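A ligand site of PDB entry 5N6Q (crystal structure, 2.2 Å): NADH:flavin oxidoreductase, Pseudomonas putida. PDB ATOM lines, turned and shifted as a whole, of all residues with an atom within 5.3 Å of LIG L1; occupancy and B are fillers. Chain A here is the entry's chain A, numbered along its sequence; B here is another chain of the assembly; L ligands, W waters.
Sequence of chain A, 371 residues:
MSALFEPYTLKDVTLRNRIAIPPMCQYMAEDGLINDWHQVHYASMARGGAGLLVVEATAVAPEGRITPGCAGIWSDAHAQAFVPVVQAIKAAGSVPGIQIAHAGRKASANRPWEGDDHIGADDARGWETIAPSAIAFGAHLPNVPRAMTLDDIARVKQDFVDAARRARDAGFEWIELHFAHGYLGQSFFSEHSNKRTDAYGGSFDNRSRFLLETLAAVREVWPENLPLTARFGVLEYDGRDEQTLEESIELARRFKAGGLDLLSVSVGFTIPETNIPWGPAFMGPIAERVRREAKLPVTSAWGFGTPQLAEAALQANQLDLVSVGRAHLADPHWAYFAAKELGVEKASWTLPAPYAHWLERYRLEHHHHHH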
ATOM      1  N   PRO A  22      35.134  22.062  13.093  1.00  0.00           N
ATOM      2  CA  PRO A  22      34.260  22.135  14.268  1.00  0.00           C
ATOM      3  C   PRO A  22      33.697  20.772  14.593  1.00  0.00           C
ATOM      4  O   PRO A  22      33.779  19.852  13.755  1.00  0.00           O
ATOM      5  CB  PRO A  22      33.166  23.113  13.818  1.00  0.00           C
ATOM      6  CG  PRO A  22      33.043  22.818  12.359  1.00  0.00           C
ATOM      7  CD  PRO A  22      34.461  22.544  11.880  1.00  0.00           C
ATOM      8  N   PRO A  23      33.131  20.583  15.780  1.00  0.00           N
ATOM      9  CA  PRO A  23      32.582  19.256  16.128  1.00  0.00           C
ATOM     10  C   PRO A  23      31.388  18.920  15.260  1.00  0.00           C
ATOM     11  O   PRO A  23      30.485  19.725  15.096  1.00  0.00           O
ATOM     12  CB  PRO A  23      32.180  19.420  17.606  1.00  0.00           C
ATOM     13  CG  PRO A  23      32.013  20.935  17.795  1.00  0.00           C
ATOM     14  CD  PRO A  23      33.072  21.532  16.904  1.00  0.00           C
ATOM     15  N   MET A  24      31.365  17.688  14.722  1.00  0.00           N
ATOM     16  CA  MET A  24      30.249  17.286  13.876  1.00  0.00           C
ATOM     17  C   MET A  24      29.876  15.861  14.221  1.00  0.00           C
ATOM     18  O   MET A  24      30.621  14.925  13.894  1.00  0.00           O
ATOM     19  CB  MET A  24      30.581  17.423  12.384  1.00  0.00           C
ATOM     20  CG  MET A  24      30.714  18.836  11.945  1.00  0.00           C
ATOM     21  SD  MET A  24      31.186  19.010  10.209  1.00  0.00           S
ATOM     22  CE  MET A  24      32.883  18.474  10.250  1.00  0.00           C
ATOM     23  N   CYS A  25      28.740  15.678  14.903  1.00  0.00           N
ATOM     24  CA  CYS A  25      28.321  14.327  15.273  1.00  0.00           C
ATOM     25  C   CYS A  25      28.111  13.484  14.033  1.00  0.00           C
ATOM     26  O   CYS A  25      27.617  13.961  13.010  1.00  0.00           O
ATOM     27  CB  CYS A  25      27.043  14.320  16.119  1.00  0.00           C
ATOM     28  SG  CYS A  25      26.476  12.595  16.538  1.00  0.00           S
ATOM     29  N   GLN A  26      28.470  12.215  14.157  1.00  0.00           N
ATOM     30  CA  GLN A  26      28.469  11.264  13.067  1.00  0.00           C
ATOM     31  C   GLN A  26      27.323  10.268  13.136  1.00  0.00           C
ATOM     32  O   GLN A  26      27.023   9.620  12.130  1.00  0.00           O
ATOM     33  CB  GLN A  26      29.816  10.533  13.055  1.00  0.00           C
ATOM     34  CG  GLN A  26      30.983  11.433  12.654  1.00  0.00           C
ATOM     35  CD  GLN A  26      30.755  12.131  11.294  1.00  0.00           C
ATOM     36  OE1 GLN A  26      30.838  11.499  10.242  1.00  0.00           O
ATOM     37  NE2 GLN A  26      30.472  13.428  11.323  1.00  0.00           N
ATOM     38  N   TYR A  27      26.651  10.164  14.269  1.00  0.00           N
ATOM     39  CA  TYR A  27      25.511   9.266  14.454  1.00  0.00           C
ATOM     40  C   TYR A  27      25.899   7.800  14.200  1.00  0.00           C
ATOM     41  O   TYR A  27      25.066   6.950  13.921  1.00  0.00           O
ATOM     42  CB  TYR A  27      24.334   9.714  13.582  1.00  0.00           C
ATOM     43  CG  TYR A  27      24.016  11.183  13.816  1.00  0.00           C
ATOM     44  CD1 TYR A  27      23.371  11.606  14.984  1.00  0.00           C
ATOM     45  CD2 TYR A  27      24.411  12.162  12.906  1.00  0.00           C
ATOM     46  CE1 TYR A  27      23.113  12.943  15.214  1.00  0.00           C
ATOM     47  CE2 TYR A  27      24.142  13.505  13.131  1.00  0.00           C
ATOM     48  CZ  TYR A  27      23.495  13.886  14.280  1.00  0.00           C
ATOM     49  OH  TYR A  27      23.247  15.225  14.510  1.00  0.00           O
ATOM     50  N   GLU A  56      33.476  15.507  17.548  1.00  0.00           N
ATOM     51  CA  GLU A  56      32.054  15.718  17.744  1.00  0.00           C
ATOM     52  C   GLU A  56      31.564  15.719  19.200  1.00  0.00           C
ATOM     53  O   GLU A  56      32.205  15.151  20.094  1.00  0.00           O
ATOM     54  CB  GLU A  56      31.300  14.617  17.020  1.00  0.00           C
ATOM     55  CG  GLU A  56      31.551  13.244  17.650  1.00  0.00           C
ATOM     56  CD  GLU A  56      31.093  12.098  16.738  1.00  0.00           C
ATOM     57  OE1 GLU A  56      31.917  11.584  15.945  1.00  0.00           O
ATOM     58  OE2 GLU A  56      29.903  11.743  16.795  1.00  0.00           O
ATOM     59  N   ALA A  57      30.365  16.263  19.401  1.00  0.00           N
ATOM     60  CA  ALA A  57      29.729  16.322  20.704  1.00  0.00           C
ATOM     61  C   ALA A  57      29.705  14.949  21.379  1.00  0.00           C
ATOM     62  O   ALA A  57      29.064  14.012  20.896  1.00  0.00           O
ATOM     63  CB  ALA A  57      28.305  16.839  20.530  1.00  0.00           C
ATOM     64  N   GLN A  99      34.694  18.114  22.064  1.00  0.00           N
ATOM     65  CA  GLN A  99      33.567  18.817  22.660  1.00  0.00           C
ATOM     66  C   GLN A  99      32.830  17.850  23.573  1.00  0.00           C
ATOM     67  O   GLN A  99      32.359  16.808  23.128  1.00  0.00           O
ATOM     68  CB  GLN A  99      32.625  19.347  21.582  1.00  0.00           C
ATOM     69  CG  GLN A  99      31.446  20.083  22.120  1.00  0.00           C
ATOM     70  CD  GLN A  99      30.468  20.442  21.008  1.00  0.00           C
ATOM     71  OE1 GLN A  99      29.842  19.553  20.450  1.00  0.00           O
ATOM     72  NE2 GLN A  99      30.329  21.731  20.688  1.00  0.00           N
ATOM     73  N   GLU A 176      36.396  21.570  24.694  1.00  0.00           N
ATOM     74  CA  GLU A 176      35.355  22.546  24.416  1.00  0.00           C
ATOM     75  C   GLU A 176      34.120  22.154  25.215  1.00  0.00           C
ATOM     76  O   GLU A 176      33.602  21.039  25.053  1.00  0.00           O
ATOM     77  CB  GLU A 176      35.008  22.593  22.918  1.00  0.00           C
ATOM     78  CG  GLU A 176      33.943  23.637  22.521  1.00  0.00           C
ATOM     79  CD  GLU A 176      33.688  23.723  20.976  1.00  0.00           C
ATOM     80  OE1 GLU A 176      34.621  24.091  20.202  1.00  0.00           O
ATOM     81  OE2 GLU A 176      32.555  23.424  20.534  1.00  0.00           O
ATOM     82  N   HIS A 178      30.254  22.267  25.724  1.00  0.00           N
ATOM     83  CA  HIS A 178      29.133  22.554  24.831  1.00  0.00           C
ATOM     84  C   HIS A 178      28.047  23.305  25.599  1.00  0.00           C
ATOM     85  O   HIS A 178      27.082  22.723  26.091  1.00  0.00           O
ATOM     86  CB  HIS A 178      28.580  21.280  24.215  1.00  0.00           C
ATOM     87  CG  HIS A 178      27.764  21.522  22.970  1.00  0.00           C
ATOM     88  ND1 HIS A 178      27.397  22.787  22.554  1.00  0.00           N
ATOM     89  CD2 HIS A 178      27.330  20.664  22.013  1.00  0.00           C
ATOM     90  CE1 HIS A 178      26.719  22.682  21.420  1.00  0.00           C
ATOM     91  NE2 HIS A 178      26.676  21.410  21.065  1.00  0.00           N
ATOM     92  N   HIS A 181      23.542  25.832  21.484  1.00  0.00           N
ATOM     93  CA  HIS A 181      22.590  25.072  20.646  1.00  0.00           C
ATOM     94  C   HIS A 181      21.416  24.503  21.451  1.00  0.00           C
ATOM     95  O   HIS A 181      20.830  23.487  21.062  1.00  0.00           O
ATOM     96  CB  HIS A 181      23.283  23.961  19.850  1.00  0.00           C
ATOM     97  CG  HIS A 181      24.347  24.477  18.922  1.00  0.00           C
ATOM     98  ND1 HIS A 181      25.242  23.649  18.271  1.00  0.00           N
ATOM     99  CD2 HIS A 181      24.685  25.737  18.564  1.00  0.00           C
ATOM    100  CE1 HIS A 181      26.068  24.373  17.547  1.00  0.00           C
ATOM    101  NE2 HIS A 181      25.758  25.649  17.705  1.00  0.00           N
ATOM    102  N   ARG A 231      31.828  26.469  23.559  1.00  0.00           N
ATOM    103  CA  ARG A 231      30.943  26.931  22.491  1.00  0.00           C
ATOM    104  C   ARG A 231      29.679  27.443  23.159  1.00  0.00           C
ATOM    105  O   ARG A 231      29.167  26.801  24.083  1.00  0.00           O
ATOM    106  CB  ARG A 231      30.598  25.811  21.508  1.00  0.00           C
ATOM    107  CG  ARG A 231      29.812  26.295  20.305  1.00  0.00           C
ATOM    108  CD  ARG A 231      29.751  25.245  19.196  1.00  0.00           C
ATOM    109  NE  ARG A 231      30.018  25.861  17.905  1.00  0.00           N
ATOM    110  CZ  ARG A 231      29.939  25.236  16.740  1.00  0.00           C
ATOM    111  NH1 ARG A 231      29.592  23.942  16.688  1.00  0.00           N
ATOM    112  NH2 ARG A 231      30.248  25.899  15.621  1.00  0.00           N
ATOM    113  N   ALA A 301      31.540  29.679  12.863  1.00  0.00           N
ATOM    114  CA  ALA A 301      31.285  28.759  11.769  1.00  0.00           C
ATOM    115  C   ALA A 301      30.003  29.173  11.052  1.00  0.00           C
ATOM    116  O   ALA A 301      29.301  30.084  11.481  1.00  0.00           O
ATOM    117  CB  ALA A 301      31.197  27.309  12.293  1.00  0.00           C
ATOM    118  N   TRP A 302      29.731  28.468   9.953  1.00  0.00           N
ATOM    119  CA  TRP A 302      28.607  28.576   9.036  1.00  0.00           C
ATOM    120  C   TRP A 302      29.019  29.337   7.775  1.00  0.00           C
ATOM    121  O   TRP A 302      29.014  30.571   7.745  1.00  0.00           O
ATOM    122  CB  TRP A 302      27.362  29.255   9.625  1.00  0.00           C
ATOM    123  CG  TRP A 302      26.202  29.005   8.641  1.00  0.00           C
ATOM    124  CD1 TRP A 302      25.921  29.726   7.487  1.00  0.00           C
ATOM    125  CD2 TRP A 302      25.256  27.933   8.678  1.00  0.00           C
ATOM    126  NE1 TRP A 302      24.831  29.176   6.839  1.00  0.00           N
ATOM    127  CE2 TRP A 302      24.398  28.079   7.555  1.00  0.00           C
ATOM    128  CE3 TRP A 302      25.021  26.875   9.566  1.00  0.00           C
ATOM    129  CZ2 TRP A 302      23.345  27.215   7.301  1.00  0.00           C
ATOM    130  CZ3 TRP A 302      23.975  26.025   9.327  1.00  0.00           C
ATOM    131  CH2 TRP A 302      23.155  26.182   8.188  1.00  0.00           C
ATOM    132  N   GLY A 303      29.336  28.582   6.718  1.00  0.00           N
ATOM    133  CA  GLY A 303      29.576  29.130   5.402  1.00  0.00           C
ATOM    134  C   GLY A 303      30.990  29.555   5.097  1.00  0.00           C
ATOM    135  O   GLY A 303      31.183  30.279   4.123  1.00  0.00           O
ATOM    136  N   PHE A 304      31.975  29.162   5.892  1.00  0.00           N
ATOM    137  CA  PHE A 304      33.346  29.560   5.617  1.00  0.00           C
ATOM    138  C   PHE A 304      34.066  28.565   4.694  1.00  0.00           C
ATOM    139  O   PHE A 304      35.286  28.663   4.525  1.00  0.00           O
ATOM    140  CB  PHE A 304      34.107  29.763   6.939  1.00  0.00           C
ATOM    141  CG  PHE A 304      33.635  30.988   7.733  1.00  0.00           C
ATOM    142  CD1 PHE A 304      34.061  32.272   7.392  1.00  0.00           C
ATOM    143  CD2 PHE A 304      32.815  30.854   8.848  1.00  0.00           C
ATOM    144  CE1 PHE A 304      33.661  33.389   8.127  1.00  0.00           C
ATOM    145  CE2 PHE A 304      32.406  31.967   9.598  1.00  0.00           C
ATOM    146  CZ  PHE A 304      32.822  33.244   9.235  1.00  0.00           C
ATOM    147  N   GLY A 305      33.330  27.643   4.086  1.00  0.00           N
ATOM    148  CA  GLY A 305      33.910  26.748   3.106  1.00  0.00           C
ATOM    149  C   GLY A 305      34.384  27.414   1.838  1.00  0.00           C
ATOM    150  O   GLY A 305      35.054  26.759   1.024  1.00  0.00           O
ATOM    151  N   SER A 323      36.203  28.072  11.668  1.00  0.00           N
ATOM    152  CA  SER A 323      35.693  26.709  11.717  1.00  0.00           C
ATOM    153  C   SER A 323      34.973  26.375  10.400  1.00  0.00           C
ATOM    154  O   SER A 323      34.053  27.095   9.995  1.00  0.00           O
ATOM    155  CB  SER A 323      34.791  26.509  12.925  1.00  0.00           C
ATOM    156  OG  SER A 323      35.540  26.687  14.124  1.00  0.00           O
ATOM    157  N   VAL A 324      35.421  25.297   9.743  1.00  0.00           N
ATOM    158  CA  VAL A 324      34.919  24.819   8.451  1.00  0.00           C
ATOM    159  C   VAL A 324      34.392  23.408   8.689  1.00  0.00           C
ATOM    160  O   VAL A 324      35.170  22.480   8.873  1.00  0.00           O
ATOM    161  CB  VAL A 324      36.029  24.822   7.383  1.00  0.00           C
ATOM    162  CG1 VAL A 324      35.539  24.309   5.979  1.00  0.00           C
ATOM    163  CG2 VAL A 324      36.648  26.225   7.264  1.00  0.00           C
ATOM    164  N   GLY A 325      33.073  23.244   8.683  1.00  0.00           N
ATOM    165  CA  GLY A 325      32.503  21.937   8.949  1.00  0.00           C
ATOM    166  C   GLY A 325      32.131  21.093   7.731  1.00  0.00           C
ATOM    167  O   GLY A 325      32.869  20.171   7.341  1.00  0.00           O
ATOM    168  N   ARG A 326      30.991  21.409   7.120  1.00  0.00           N
ATOM    169  CA  ARG A 326      30.436  20.597   6.036  1.00  0.00           C
ATOM    170  C   ARG A 326      31.377  20.490   4.844  1.00  0.00           C
ATOM    171  O   ARG A 326      31.369  19.462   4.146  1.00  0.00           O
ATOM    172  CB  ARG A 326      29.070  21.142   5.603  1.00  0.00           C
ATOM    173  CG  ARG A 326      27.902  20.660   6.479  1.00  0.00           C
ATOM    174  CD  ARG A 326      26.643  21.470   6.220  1.00  0.00           C
ATOM    175  NE  ARG A 326      26.881  22.869   6.548  1.00  0.00           N
ATOM    176  CZ  ARG A 326      25.969  23.830   6.464  1.00  0.00           C
ATOM    177  NH1 ARG A 326      24.746  23.529   6.051  1.00  0.00           N
ATOM    178  NH2 ARG A 326      26.275  25.062   6.777  1.00  0.00           N
ATOM    179  N   ALA A 327      32.173  21.520   4.566  1.00  0.00           N
ATOM    180  CA  ALA A 327      33.108  21.424   3.455  1.00  0.00           C
ATOM    181  C   ALA A 327      34.154  20.328   3.699  1.00  0.00           C
ATOM    182  O   ALA A 327      34.679  19.769   2.728  1.00  0.00           O
ATOM    183  CB  ALA A 327      33.793  22.764   3.188  1.00  0.00           C
ATOM    184  N   LEU A 329      33.356  17.520   5.295  1.00  0.00           N
ATOM    185  CA  LEU A 329      32.640  16.284   4.989  1.00  0.00           C
ATOM    186  C   LEU A 329      32.666  16.004   3.498  1.00  0.00           C
ATOM    187  O   LEU A 329      32.933  14.882   3.059  1.00  0.00           O
ATOM    188  CB  LEU A 329      31.195  16.368   5.489  1.00  0.00           C
ATOM    189  CG  LEU A 329      30.950  16.660   6.972  1.00  0.00           C
ATOM    190  CD1 LEU A 329      29.500  16.481   7.282  1.00  0.00           C
ATOM    191  CD2 LEU A 329      31.808  15.773   7.887  1.00  0.00           C
ATOM    192  N   PRO B 354      26.164   9.557   7.023  1.00  0.00           N
ATOM    193  CA  PRO B 354      26.658  10.626   7.909  1.00  0.00           C
ATOM    194  C   PRO B 354      27.171  11.861   7.156  1.00  0.00           C
ATOM    195  O   PRO B 354      27.200  12.948   7.758  1.00  0.00           O
ATOM    196  CB  PRO B 354      27.773   9.933   8.714  1.00  0.00           C
ATOM    197  CG  PRO B 354      27.418   8.448   8.659  1.00  0.00           C
ATOM    198  CD  PRO B 354      26.808   8.247   7.288  1.00  0.00           C
ATOM    199  N   TRP B 358      23.676  15.725   5.042  1.00  0.00           N
ATOM    200  CA  TRP B 358      23.990  17.123   5.264  1.00  0.00           C
ATOM    201  C   TRP B 358      24.482  17.850   4.014  1.00  0.00           C
ATOM    202  O   TRP B 358      24.552  19.081   4.020  1.00  0.00           O
ATOM    203  CB  TRP B 358      25.029  17.216   6.372  1.00  0.00           C
ATOM    204  CG  TRP B 358      24.580  16.419   7.554  1.00  0.00           C
ATOM    205  CD1 TRP B 358      24.973  15.152   7.911  1.00  0.00           C
ATOM    206  CD2 TRP B 358      23.596  16.821   8.507  1.00  0.00           C
ATOM    207  NE1 TRP B 358      24.287  14.747   9.037  1.00  0.00           N
ATOM    208  CE2 TRP B 358      23.436  15.755   9.424  1.00  0.00           C
ATOM    209  CE3 TRP B 358      22.832  17.973   8.686  1.00  0.00           C
ATOM    210  CZ2 TRP B 358      22.566  15.832  10.506  1.00  0.00           C
ATOM    211  CZ3 TRP B 358      21.955  18.030   9.746  1.00  0.00           C
ATOM    212  CH2 TRP B 358      21.835  16.966  10.652  1.00  0.00           C
HETATM  213  N1  LIG L   1      27.933  21.545  16.311  1.00  0.00           N
HETATM  214  C1  LIG L   1      28.304  21.232  17.574  1.00  0.00           C
HETATM  215  O1  LIG L   1      28.460  22.106  18.436  1.00  0.00           O
HETATM  216  N2  LIG L   1      28.453  19.906  17.925  1.00  0.00           N
HETATM  217  C2  LIG L   1      28.224  18.821  17.106  1.00  0.00           C
HETATM  218  O2  LIG L   1      28.562  17.704  17.453  1.00  0.00           O
HETATM  219  C3  LIG L   1      27.742  19.163  15.819  1.00  0.00           C
HETATM  220  N3  LIG L   1      27.476  18.195  14.994  1.00  0.00           N
HETATM  221  C4  LIG L   1      27.151  18.522  13.699  1.00  0.00           C
HETATM  222  C5  LIG L   1      26.978  17.481  12.800  1.00  0.00           C
HETATM  223  C6  LIG L   1      26.769  17.737  11.446  1.00  0.00           C
HETATM  224  C7  LIG L   1      26.690  16.578  10.485  1.00  0.00           C
HETATM  225  C8  LIG L   1      26.683  19.067  10.997  1.00  0.00           C
HETATM  226  C9  LIG L   1      26.433  19.384   9.552  1.00  0.00           C
HETATM  227  C10 LIG L   1      26.838  20.103  11.911  1.00  0.00           C
HETATM  228  C11 LIG L   1      27.087  19.849  13.255  1.00  0.00           C
HETATM  229  N4  LIG L   1      27.368  20.874  14.178  1.00  0.00           N
HETATM  230  C12 LIG L   1      27.669  20.563  15.483  1.00  0.00           C
HETATM  231  C13 LIG L   1      27.547  22.263  13.726  1.00  0.00           C
HETATM  232  C14 LIG L   1      28.940  22.470  13.130  1.00  0.00           C
HETATM  233  O3  LIG L   1      29.949  22.398  14.147  1.00  0.00           O
HETATM  234  C15 LIG L   1      29.103  23.806  12.411  1.00  0.00           C
HETATM  235  O4  LIG L   1      29.014  24.879  13.357  1.00  0.00           O
HETATM  236  C16 LIG L   1      28.079  24.052  11.305  1.00  0.00           C
HETATM  237  O5  LIG L   1      28.019  22.897  10.472  1.00  0.00           O
HETATM  238  C17 LIG L   1      28.365  25.321  10.511  1.00  0.00           C
HETATM  239  O6  LIG L   1      29.612  25.233   9.801  1.00  0.00           O
HETATM  240  P1  LIG L   1      29.708  24.759   8.227  1.00  0.00           P
HETATM  241  O7  LIG L   1      29.252  23.344   8.131  1.00  0.00           O
HETATM  242  O8  LIG L   1      28.834  25.757   7.453  1.00  0.00           O
HETATM  243  O9  LIG L   1      31.120  24.974   7.781  1.00  0.00           O
HETATM  244  C1  LG2 L   2      23.709  20.458  13.669  1.00  0.00           C
HETATM  245  C2  LG2 L   2      23.267  19.287  13.075  1.00  0.00           C
HETATM  246  C3  LG2 L   2      23.315  18.103  13.762  1.00  0.00           C
HETATM  247  C4  LG2 L   2      23.799  18.072  15.071  1.00  0.00           C
HETATM  248  C5  LG2 L   2      24.615  20.538  17.833  1.00  0.00           C
HETATM  249  C6  LG2 L   2      25.035  18.109  17.718  1.00  0.00           C
HETATM  250  O1  LG2 L   2      25.545  20.940  18.517  1.00  0.00           O
HETATM  251  C7  LG2 L   2      24.659  19.226  17.110  1.00  0.00           C
HETATM  252  C8  LG2 L   2      24.233  19.238  15.694  1.00  0.00           C
HETATM  253  C9  LG2 L   2      24.202  20.431  14.964  1.00  0.00           C
HETATM  254  O2  LG2 L   2      23.493  21.221  17.677  1.00  0.00           O
HETATM  255  O   HOH W   1      32.073  24.338   5.268  1.00  0.00           O
HETATM  256  O   HOH W   2      28.560  25.389   4.703  1.00  0.00           O
HETATM  257  O   HOH W   3      31.877  27.398   8.291  1.00  0.00           O
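A nitrogen (N3) of LIG L1 sits at hydrogen-bond distance from the backbone NH of Cys 25, at 2.8 Å.
O3 of LIG L1 sits at hydrogen-bond distance from O of Pro 23 (2.9 Å).
The backbone NH of Trp 302 sits at hydrogen-bond distance from an oxygen (O6) of LIG L1 (3.2 Å).
O4 of LIG L1 is in hydrogen-bond range of NH2 of Arg 231 (2.8 Å).
OE1 of Gln 99 lies within hydrogen-bond range of N2 of LIG L1 (2.9 Å).
The backbone NH of Gly 303 is in hydrogen-bond range of an oxygen (O8) of LIG L1, 3.0 Å away.
An oxygen (O1) of LIG L1 lies within hydrogen-bond range of a ring nitrogen (NE2) of His 178 (3.3 Å).
O1 of LG2 L2 lies within hydrogen-bond range of NE2 of His 178 (2.8 Å).
The backbone NH (N) of Gly 325 lies within hydrogen-bond range of an oxygen (O9) of LIG L1 (2.8 Å).
The guanidinium group (NH2) of Arg 326 lies within salt-bridge range of an oxygen (O8) of LIG L1, at 2.7 Å.
N of Ala 57 lies within hydrogen-bond range of O2 of LIG L1 (3.0 Å).
An oxygen (O1) of LG2 L2 sits at hydrogen-bond distance from a ring nitrogen (ND1) of His 181, 2.7 Å away.
The backbone NH of Arg 326 is in hydrogen-bond range of an oxygen (O7) of LIG L1.
A nitrogen (N2) of LIG L1 sits close to an oxygen (O1) of LG2 L2.
The side-chain carboxylate of Glu 176 sits at hydrogen-bond distance from the side-chain amide nitrogen of Gln 99 (2.8 Å).
The side-chain sulfur (SG) of Cys 25 sits at hydrogen-bond distance from the backbone NH (N) of Tyr 27 (3.3 Å).
SG of Cys 25 lies close to OE2 of Glu 56, 3.5 Å away.
The backbone carbonyl oxygen (O) of Met 24 lies within hydrogen-bond range of the side-chain amide nitrogen (NE2) of Gln 26 (3.0 Å).
N of Ala 57 lies close to OE1 of Gln 99 (3.5 Å).
Pro 22 touches LIG L1.
Met 24 touches LIG L1 (CA to N3, 3.1 Å).
His 181 touches LIG L1.
CB of Ala 301 touches O4 of LIG L1, at 3.4 Å.
Val 324 touches LIG L1 (C to O9, 3.7 Å).
NE1 of Trp 358 of chain B touches C7 of LIG L1, at 3.4 Å.
Hydrophobic or aromatic side chains within 4 Å of LIG L1: Pro 22, Pro 23, Met 24, Ala 57, His 178, His 181, Ala 301, Trp 302 and Trp 358 of chain B.
Within 4 Å of LIG L1: Pro 22, Pro 23, Met 24, Cys 25, Ala 57, Gln 99, His 178, His 181, Arg 231, Ala 301, Trp 302, Gly 303, Val 324, Gly 325, Arg 326 and Trp 358 of chain B.
The nearest printed residue that does not touch LIG L1 is Glu 56 (4.001 Å).
Water W1 lies within hydrogen-bond range of O9 of LIG L1 and N of Ala 327.
Water W2 bridges O8 of LIG L1 (2.8 Å) and NH2 of Arg 326 (3.1 Å).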
